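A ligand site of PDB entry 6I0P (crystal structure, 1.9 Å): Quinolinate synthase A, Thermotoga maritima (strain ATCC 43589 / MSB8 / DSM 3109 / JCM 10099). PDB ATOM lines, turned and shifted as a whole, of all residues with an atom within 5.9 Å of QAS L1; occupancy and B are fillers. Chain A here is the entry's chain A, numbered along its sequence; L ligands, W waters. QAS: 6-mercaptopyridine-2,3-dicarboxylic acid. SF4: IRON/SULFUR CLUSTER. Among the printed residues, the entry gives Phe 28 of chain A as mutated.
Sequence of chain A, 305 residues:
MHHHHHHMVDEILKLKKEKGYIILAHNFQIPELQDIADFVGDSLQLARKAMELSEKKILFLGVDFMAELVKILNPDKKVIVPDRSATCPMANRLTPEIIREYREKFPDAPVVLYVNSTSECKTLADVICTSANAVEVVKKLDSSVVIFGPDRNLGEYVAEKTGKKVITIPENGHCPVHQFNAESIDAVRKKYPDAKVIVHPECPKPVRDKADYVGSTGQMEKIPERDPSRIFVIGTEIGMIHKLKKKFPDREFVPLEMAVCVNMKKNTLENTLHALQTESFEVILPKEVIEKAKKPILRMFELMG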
ATOM      1  N   HIS A  26     -19.475  21.924  -4.823  1.00  0.00           N
ATOM      2  CA  HIS A  26     -20.674  22.319  -4.076  1.00  0.00           C
ATOM      3  C   HIS A  26     -21.465  23.359  -4.885  1.00  0.00           C
ATOM      4  O   HIS A  26     -20.897  24.106  -5.710  1.00  0.00           O
ATOM      5  CB  HIS A  26     -20.296  22.860  -2.701  1.00  0.00           C
ATOM      6  CG  HIS A  26     -21.477  23.032  -1.819  1.00  0.00           C
ATOM      7  ND1 HIS A  26     -22.150  24.241  -1.704  1.00  0.00           N
ATOM      8  CD2 HIS A  26     -22.102  22.162  -1.003  1.00  0.00           C
ATOM      9  CE1 HIS A  26     -23.147  24.104  -0.871  1.00  0.00           C
ATOM     10  NE2 HIS A  26     -23.148  22.833  -0.413  1.00  0.00           N
ATOM     11  N   ASN A  27     -22.765  23.420  -4.600  1.00  0.00           N
ATOM     12  CA  ASN A  27     -23.726  24.351  -5.185  1.00  0.00           C
ATOM     13  C   ASN A  27     -23.291  25.804  -4.983  1.00  0.00           C
ATOM     14  O   ASN A  27     -23.758  26.647  -5.748  1.00  0.00           O
ATOM     15  CB  ASN A  27     -25.107  24.135  -4.563  1.00  0.00           C
ATOM     16  CG  ASN A  27     -25.757  22.846  -5.029  1.00  0.00           C
ATOM     17  OD1 ASN A  27     -25.498  22.373  -6.137  1.00  0.00           O
ATOM     18  ND2 ASN A  27     -26.588  22.269  -4.193  1.00  0.00           N
ATOM     19  N   PHE A  28     -22.442  26.089  -3.983  1.00  0.00           N
ATOM     20  CA  PHE A  28     -22.076  27.499  -3.671  1.00  0.00           C
ATOM     21  C   PHE A  28     -20.744  27.879  -4.317  1.00  0.00           C
ATOM     22  O   PHE A  28     -20.219  28.948  -4.058  1.00  0.00           O
ATOM     23  CB  PHE A  28     -22.066  27.761  -2.174  1.00  0.00           C
ATOM     24  CG  PHE A  28     -23.402  27.613  -1.472  1.00  0.00           C
ATOM     25  CD1 PHE A  28     -24.592  27.482  -2.173  1.00  0.00           C
ATOM     26  CD2 PHE A  28     -23.449  27.591  -0.091  1.00  0.00           C
ATOM     27  CE1 PHE A  28     -25.796  27.354  -1.498  1.00  0.00           C
ATOM     28  CE2 PHE A  28     -24.645  27.458   0.595  1.00  0.00           C
ATOM     29  CZ  PHE A  28     -25.835  27.326  -0.116  1.00  0.00           C
ATOM     30  N   GLY A  41     -23.457  19.531  -6.469  1.00  0.00           N
ATOM     31  CA  GLY A  41     -24.574  19.213  -5.594  1.00  0.00           C
ATOM     32  C   GLY A  41     -24.325  19.659  -4.171  1.00  0.00           C
ATOM     33  O   GLY A  41     -23.380  20.436  -3.907  1.00  0.00           O
ATOM     34  N   ASP A  42     -25.169  19.153  -3.285  1.00  0.00           N
ATOM     35  CA  ASP A  42     -25.022  19.438  -1.844  1.00  0.00           C
ATOM     36  C   ASP A  42     -23.984  18.477  -1.236  1.00  0.00           C
ATOM     37  O   ASP A  42     -23.474  17.590  -1.952  1.00  0.00           O
ATOM     38  CB  ASP A  42     -26.390  19.489  -1.182  1.00  0.00           C
ATOM     39  CG  ASP A  42     -27.049  18.136  -1.011  1.00  0.00           C
ATOM     40  OD1 ASP A  42     -26.332  17.131  -0.864  1.00  0.00           O
ATOM     41  OD2 ASP A  42     -28.273  18.130  -0.991  1.00  0.00           O
ATOM     42  N   SER A  43     -23.604  18.712   0.015  1.00  0.00           N
ATOM     43  CA  SER A  43     -22.448  18.020   0.639  1.00  0.00           C
ATOM     44  C   SER A  43     -22.688  16.506   0.684  1.00  0.00           C
ATOM     45  O   SER A  43     -21.784  15.731   0.336  1.00  0.00           O
ATOM     46  CB  SER A  43     -22.137  18.574   2.005  1.00  0.00           C
ATOM     47  OG  SER A  43     -23.289  18.544   2.815  1.00  0.00           O
ATOM     48  N   LEU A  44     -23.890  16.080   1.051  1.00  0.00           N
ATOM     49  CA  LEU A  44     -24.201  14.640   1.126  1.00  0.00           C
ATOM     50  C   LEU A  44     -24.339  14.045  -0.277  1.00  0.00           C
ATOM     51  O   LEU A  44     -23.886  12.916  -0.500  1.00  0.00           O
ATOM     52  CB  LEU A  44     -25.467  14.417   1.939  1.00  0.00           C
ATOM     53  CG  LEU A  44     -25.698  12.955   2.330  1.00  0.00           C
ATOM     54  CD1 LEU A  44     -24.492  12.355   3.041  1.00  0.00           C
ATOM     55  CD2 LEU A  44     -26.950  12.820   3.189  1.00  0.00           C
ATOM     56  N   VAL A  63     -15.892  23.584   1.062  1.00  0.00           N
ATOM     57  CA  VAL A  63     -15.175  23.973   2.291  1.00  0.00           C
ATOM     58  C   VAL A  63     -14.814  22.698   3.044  1.00  0.00           C
ATOM     59  O   VAL A  63     -15.349  21.623   2.715  1.00  0.00           O
ATOM     60  CB  VAL A  63     -16.006  24.925   3.177  1.00  0.00           C
ATOM     61  CG1 VAL A  63     -16.189  26.291   2.497  1.00  0.00           C
ATOM     62  CG2 VAL A  63     -17.311  24.287   3.568  1.00  0.00           C
ATOM     63  N   PHE A  65     -15.166  20.956   5.899  1.00  0.00           N
ATOM     64  CA  PHE A  65     -15.968  19.907   6.584  1.00  0.00           C
ATOM     65  C   PHE A  65     -16.552  18.989   5.514  1.00  0.00           C
ATOM     66  O   PHE A  65     -16.759  17.826   5.808  1.00  0.00           O
ATOM     67  CB  PHE A  65     -17.022  20.481   7.543  1.00  0.00           C
ATOM     68  CG  PHE A  65     -18.251  21.058   6.887  1.00  0.00           C
ATOM     69  CD1 PHE A  65     -19.256  20.224   6.390  1.00  0.00           C
ATOM     70  CD2 PHE A  65     -18.412  22.421   6.743  1.00  0.00           C
ATOM     71  CE1 PHE A  65     -20.378  20.747   5.760  1.00  0.00           C
ATOM     72  CE2 PHE A  65     -19.527  22.948   6.091  1.00  0.00           C
ATOM     73  CZ  PHE A  65     -20.516  22.105   5.616  1.00  0.00           C
ATOM     74  N   MET A  66     -16.828  19.519   4.326  1.00  0.00           N
ATOM     75  CA  MET A  66     -17.462  18.763   3.222  1.00  0.00           C
ATOM     76  C   MET A  66     -16.443  17.868   2.556  1.00  0.00           C
ATOM     77  O   MET A  66     -16.777  16.726   2.232  1.00  0.00           O
ATOM     78  CB  MET A  66     -18.001  19.684   2.123  1.00  0.00           C
ATOM     79  CG  MET A  66     -18.887  20.758   2.576  1.00  0.00           C
ATOM     80  SD  MET A  66     -19.483  21.748   1.174  1.00  0.00           S
ATOM     81  CE  MET A  66     -20.708  22.673   2.114  1.00  0.00           C
ATOM     82  N   CYS A  88     -16.046  26.657   7.315  1.00  0.00           N
ATOM     83  CA  CYS A  88     -17.355  27.191   7.689  1.00  0.00           C
ATOM     84  C   CYS A  88     -17.241  27.850   9.063  1.00  0.00           C
ATOM     85  O   CYS A  88     -17.048  27.175  10.072  1.00  0.00           O
ATOM     86  CB  CYS A  88     -18.378  26.065   7.663  1.00  0.00           C
ATOM     87  SG  CYS A  88     -20.011  26.541   8.306  1.00  0.00           S
ATOM     88  N   TYR A 114     -25.807  18.920  12.754  1.00  0.00           N
ATOM     89  CA  TYR A 114     -25.956  19.325  11.350  1.00  0.00           C
ATOM     90  C   TYR A 114     -24.631  18.968  10.655  1.00  0.00           C
ATOM     91  O   TYR A 114     -23.540  19.105  11.235  1.00  0.00           O
ATOM     92  CB  TYR A 114     -26.303  20.810  11.353  1.00  0.00           C
ATOM     93  CG  TYR A 114     -26.564  21.454  10.006  1.00  0.00           C
ATOM     94  CD1 TYR A 114     -27.178  20.749   8.985  1.00  0.00           C
ATOM     95  CD2 TYR A 114     -26.244  22.776   9.807  1.00  0.00           C
ATOM     96  CE1 TYR A 114     -27.435  21.348   7.766  1.00  0.00           C
ATOM     97  CE2 TYR A 114     -26.497  23.397   8.585  1.00  0.00           C
ATOM     98  CZ  TYR A 114     -27.087  22.673   7.566  1.00  0.00           C
ATOM     99  OH  TYR A 114     -27.347  23.235   6.343  1.00  0.00           O
ATOM    100  N   VAL A 115     -24.714  18.514   9.421  1.00  0.00           N
ATOM    101  CA  VAL A 115     -23.514  18.104   8.666  1.00  0.00           C
ATOM    102  C   VAL A 115     -22.523  19.273   8.575  1.00  0.00           C
ATOM    103  O   VAL A 115     -21.305  19.040   8.410  1.00  0.00           O
ATOM    104  CB  VAL A 115     -23.922  17.571   7.280  1.00  0.00           C
ATOM    105  CG1 VAL A 115     -24.489  18.679   6.395  1.00  0.00           C
ATOM    106  CG2 VAL A 115     -22.771  16.833   6.637  1.00  0.00           C
ATOM    107  N   ASN A 116     -23.007  20.515   8.710  1.00  0.00           N
ATOM    108  CA  ASN A 116     -22.151  21.721   8.739  1.00  0.00           C
ATOM    109  C   ASN A 116     -21.570  21.824  10.146  1.00  0.00           C
ATOM    110  O   ASN A 116     -22.132  22.551  11.040  1.00  0.00           O
ATOM    111  CB  ASN A 116     -22.917  22.989   8.320  1.00  0.00           C
ATOM    112  CG  ASN A 116     -23.554  22.947   6.935  1.00  0.00           C
ATOM    113  OD1 ASN A 116     -23.927  21.879   6.419  1.00  0.00           O
ATOM    114  ND2 ASN A 116     -23.717  24.101   6.307  1.00  0.00           N
ATOM    115  N   THR A 130     -28.801  16.483   7.682  1.00  0.00           N
ATOM    116  CA  THR A 130     -28.728  17.547   6.647  1.00  0.00           C
ATOM    117  C   THR A 130     -29.926  18.462   6.829  1.00  0.00           C
ATOM    118  O   THR A 130     -30.843  18.108   7.583  1.00  0.00           O
ATOM    119  CB  THR A 130     -28.761  16.970   5.228  1.00  0.00           C
ATOM    120  OG1 THR A 130     -30.019  16.317   4.994  1.00  0.00           O
ATOM    121  CG2 THR A 130     -27.615  15.998   4.996  1.00  0.00           C
ATOM    122  N   SER A 131     -29.918  19.599   6.139  1.00  0.00           N
ATOM    123  CA  SER A 131     -31.073  20.521   6.187  1.00  0.00           C
ATOM    124  C   SER A 131     -32.313  19.834   5.613  1.00  0.00           C
ATOM    125  O   SER A 131     -33.401  20.113   6.122  1.00  0.00           O
ATOM    126  CB  SER A 131     -30.786  21.842   5.533  1.00  0.00           C
ATOM    127  OG  SER A 131     -30.419  21.693   4.181  1.00  0.00           O
ATOM    128  N   HIS A 178     -27.316  33.412   5.434  1.00  0.00           N
ATOM    129  CA  HIS A 178     -28.773  33.222   5.325  1.00  0.00           C
ATOM    130  C   HIS A 178     -29.561  34.224   6.182  1.00  0.00           C
ATOM    131  O   HIS A 178     -30.772  34.021   6.313  1.00  0.00           O
ATOM    132  CB  HIS A 178     -29.134  31.768   5.688  1.00  0.00           C
ATOM    133  CG  HIS A 178     -28.779  30.801   4.613  1.00  0.00           C
ATOM    134  ND1 HIS A 178     -27.558  30.162   4.570  1.00  0.00           N
ATOM    135  CD2 HIS A 178     -29.414  30.465   3.475  1.00  0.00           C
ATOM    136  CE1 HIS A 178     -27.495  29.420   3.458  1.00  0.00           C
ATOM    137  NE2 HIS A 178     -28.618  29.573   2.773  1.00  0.00           N
ATOM    138  N   HIS A 200     -34.069  28.857   2.626  1.00  0.00           N
ATOM    139  CA  HIS A 200     -33.352  27.831   3.403  1.00  0.00           C
ATOM    140  C   HIS A 200     -33.901  27.789   4.829  1.00  0.00           C
ATOM    141  O   HIS A 200     -34.263  28.815   5.389  1.00  0.00           O
ATOM    142  CB  HIS A 200     -31.838  28.098   3.398  1.00  0.00           C
ATOM    143  CG  HIS A 200     -31.066  26.849   3.651  1.00  0.00           C
ATOM    144  ND1 HIS A 200     -30.869  26.360   4.936  1.00  0.00           N
ATOM    145  CD2 HIS A 200     -30.505  25.963   2.802  1.00  0.00           C
ATOM    146  CE1 HIS A 200     -30.216  25.212   4.853  1.00  0.00           C
ATOM    147  NE2 HIS A 200     -29.996  24.943   3.553  1.00  0.00           N
ATOM    148  N   GLU A 202     -32.047  27.482   7.393  1.00  0.00           N
ATOM    149  CA  GLU A 202     -31.087  28.305   8.145  1.00  0.00           C
ATOM    150  C   GLU A 202     -31.504  29.785   8.171  1.00  0.00           C
ATOM    151  O   GLU A 202     -30.859  30.559   8.908  1.00  0.00           O
ATOM    152  CB  GLU A 202     -29.683  28.165   7.577  1.00  0.00           C
ATOM    153  CG  GLU A 202     -29.087  26.797   7.903  1.00  0.00           C
ATOM    154  CD  GLU A 202     -27.642  26.596   7.475  1.00  0.00           C
ATOM    155  OE1 GLU A 202     -26.726  27.019   8.239  1.00  0.00           O
ATOM    156  OE2 GLU A 202     -27.440  26.018   6.385  1.00  0.00           O
ATOM    157  N   GLY A 215     -36.694  24.973   2.309  1.00  0.00           N
ATOM    158  CA  GLY A 215     -36.005  23.763   1.881  1.00  0.00           C
ATOM    159  C   GLY A 215     -34.523  23.955   1.736  1.00  0.00           C
ATOM    160  O   GLY A 215     -34.059  25.088   1.552  1.00  0.00           O
ATOM    161  N   SER A 216     -33.811  22.834   1.790  1.00  0.00           N
ATOM    162  CA  SER A 216     -32.379  22.729   1.479  1.00  0.00           C
ATOM    163  C   SER A 216     -32.133  23.095   0.020  1.00  0.00           C
ATOM    164  O   SER A 216     -33.114  23.161  -0.746  1.00  0.00           O
ATOM    165  CB  SER A 216     -31.922  21.321   1.754  1.00  0.00           C
ATOM    166  OG  SER A 216     -32.374  20.451   0.744  1.00  0.00           O
ATOM    167  N   THR A 217     -30.871  23.251  -0.377  1.00  0.00           N
ATOM    168  CA  THR A 217     -30.568  23.501  -1.798  1.00  0.00           C
ATOM    169  C   THR A 217     -31.076  22.316  -2.648  1.00  0.00           C
ATOM    170  O   THR A 217     -31.599  22.555  -3.744  1.00  0.00           O
ATOM    171  CB  THR A 217     -29.094  23.855  -2.009  1.00  0.00           C
ATOM    172  OG1 THR A 217     -28.324  22.715  -1.650  1.00  0.00           O
ATOM    173  CG2 THR A 217     -28.689  25.093  -1.246  1.00  0.00           C
ATOM    174  N   GLY A 218     -30.860  21.083  -2.161  1.00  0.00           N
ATOM    175  CA  GLY A 218     -31.309  19.877  -2.866  1.00  0.00           C
ATOM    176  C   GLY A 218     -32.817  19.905  -3.058  1.00  0.00           C
ATOM    177  O   GLY A 218     -33.309  19.530  -4.143  1.00  0.00           O
ATOM    178  N   THR A 236     -31.064  31.693  -0.661  1.00  0.00           N
ATOM    179  CA  THR A 236     -29.807  31.041  -0.237  1.00  0.00           C
ATOM    180  C   THR A 236     -28.628  31.745  -0.898  1.00  0.00           C
ATOM    181  O   THR A 236     -28.796  32.833  -1.475  1.00  0.00           O
ATOM    182  CB  THR A 236     -29.872  29.520  -0.478  1.00  0.00           C
ATOM    183  OG1 THR A 236     -28.786  28.896   0.219  1.00  0.00           O
ATOM    184  CG2 THR A 236     -29.810  29.141  -1.950  1.00  0.00           C
ATOM    185  N   MET A 264     -16.645  29.885   0.562  1.00  0.00           N
ATOM    186  CA  MET A 264     -16.956  29.183  -0.689  1.00  0.00           C
ATOM    187  C   MET A 264     -16.260  29.872  -1.863  1.00  0.00           C
ATOM    188  O   MET A 264     -15.817  29.166  -2.808  1.00  0.00           O
ATOM    189  CB  MET A 264     -18.471  29.133  -0.919  1.00  0.00           C
ATOM    190  CG  MET A 264     -19.169  28.131  -0.001  1.00  0.00           C
ATOM    191  SD  MET A 264     -18.775  26.478  -0.547  1.00  0.00           S
ATOM    192  CE  MET A 264     -19.790  25.522   0.604  1.00  0.00           C
HETATM  193  O1  QAS L   1     -26.215  20.665   2.429  1.00  0.00           O
HETATM  194  C7  QAS L   1     -25.355  21.373   1.825  1.00  0.00           C
HETATM  195  O2  QAS L   1     -24.504  20.949   1.029  1.00  0.00           O
HETATM  196  C2  QAS L   1     -25.420  22.777   2.209  1.00  0.00           C
HETATM  197  N1  QAS L   1     -24.295  23.342   2.592  1.00  0.00           N
HETATM  198  C6  QAS L   1     -24.226  24.597   3.025  1.00  0.00           C
HETATM  199  S   QAS L   1     -22.626  25.095   3.337  1.00  0.00           S
HETATM  200  C5  QAS L   1     -25.344  25.410   3.130  1.00  0.00           C
HETATM  201  C4  QAS L   1     -26.579  24.864   2.726  1.00  0.00           C
HETATM  202  C3  QAS L   1     -26.656  23.549   2.281  1.00  0.00           C
HETATM  203  C8  QAS L   1     -27.901  22.921   1.729  1.00  0.00           C
HETATM  204  O4  QAS L   1     -29.025  23.397   1.945  1.00  0.00           O
HETATM  205  O3  QAS L   1     -27.715  22.093   0.758  1.00  0.00           O
HETATM  206 FE1  SF4 L   2     -23.153  29.340   5.847  1.00  0.00          FE
HETATM  207 FE2  SF4 L   2     -20.638  29.255   4.203  1.00  0.00          FE
HETATM  208 FE3  SF4 L   2     -22.487  27.167   4.353  1.00  0.00          FE
HETATM  209 FE4  SF4 L   2     -20.902  27.849   6.721  1.00  0.00          FE
HETATM  210  S1  SF4 L   2     -20.079  27.101   4.650  1.00  0.00           S
HETATM  211  S2  SF4 L   2     -23.315  27.259   6.473  1.00  0.00           S
HETATM  212  S3  SF4 L   2     -20.966  30.110   6.478  1.00  0.00           S
HETATM  213  S4  SF4 L   2     -22.952  29.163   3.492  1.00  0.00           S
HETATM  214  O   HOH W   1     -25.935  17.912   2.529  1.00  0.00           O
HETATM  215  O   HOH W   2     -28.002  21.243   4.457  1.00  0.00           O
HETATM  216  O   HOH W   3     -23.086  21.006   3.932  1.00  0.00           O
HETATM  217  O   HOH W   4     -29.484  20.173   0.233  1.00  0.00           O
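An iron atom (FE3) of SF4 L2 is bound by a sulfur (S) of QAS L1, at 2.3 Å.
Residues that only touch QAS L1: Phe 28, Asp 42, Met 66, Glu 202, Ser 216 and Met 264.
An oxygen (O4) of QAS L1 is in hydrogen-bond range of a ring nitrogen (NE2) of His 200, at 2.4 Å.
The side-chain sulfur (SG) of Cys 88 binds an iron atom (FE4) of SF4 L2 (2.2 Å).
The side-chain hydroxyl of Thr 217 is in hydrogen-bond range of an oxygen (O3) of QAS L1 (2.6 Å).
The side-chain amide nitrogen (ND2) of Asn 116 lies close to a sulfur (S) of QAS L1, at 3.3 Å.
A ring nitrogen (NE2) of His 26 sits at hydrogen-bond distance from an oxygen (O2) of QAS L1, at 2.7 Å.
The backbone NH (N) of Thr 217 lies within hydrogen-bond range of an oxygen (O4) of QAS L1 (3.0 Å).
The side-chain hydroxyl (OG) of Ser 131 lies within hydrogen-bond range of an oxygen (O4) of QAS L1, 3.1 Å away.
OG of Ser 43 lies within hydrogen-bond range of O2 of QAS L1 (3.2 Å).
The backbone NH (N) of Ser 43 lies within hydrogen-bond range of an oxygen (O2) of QAS L1, 2.6 Å away.
A sulfur (S2) of SF4 L2 lies close to the side-chain amide nitrogen of Asn 116, 3.2 Å away.
ND1 of His 200 lies within hydrogen-bond range of N of Glu 202 (2.9 Å).
The side-chain hydroxyl (OG1) of Thr 217 is in hydrogen-bond range of the side-chain amide nitrogen (ND2) of Asn 27 (3.1 Å).
The backbone NH (N) of Leu 44 lies within hydrogen-bond range of the side-chain carboxylate (OD1) of Asp 42, at 3.3 Å.
A ring nitrogen (ND1) of His 26 sits at hydrogen-bond distance from the backbone NH (N) of Phe 28, 2.9 Å away.
A ring nitrogen (NE2) of His 200 lies within hydrogen-bond range of the side-chain hydroxyl (OG) of Ser 131.
OE2 of Glu 202 is in hydrogen-bond range of OH of Tyr 114 (2.8 Å).
The side-chain hydroxyl of Ser 216 sits close to the backbone NH of Gly 218 (3.3 Å).
Water W4 lies within hydrogen-bond range of O3 of QAS L1 (2.7 Å), OD2 of Asp 42 (2.7 Å), N of Gly 218 (2.9 Å), OG of Ser 216 (2.9 Å) and OG1 of Thr 217 (3.4 Å).
Water W2 lies within hydrogen-bond range of OG of Ser 131, O1 of QAS L1 and OH of Tyr 114.
Water W1 lies within hydrogen-bond range of the side-chain hydroxyl (OG) of Ser 43 (2.7 Å), an oxygen (O1) of QAS L1 (2.8 Å) and the backbone NH (N) of Leu 44 (3.1 Å).
Water W3 lies within hydrogen-bond range of the side-chain hydroxyl of Ser 43 (2.7 Å), the side-chain amide oxygen of Asn 116 (2.8 Å) and a nitrogen (N1) of QAS L1 (3.0 Å).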
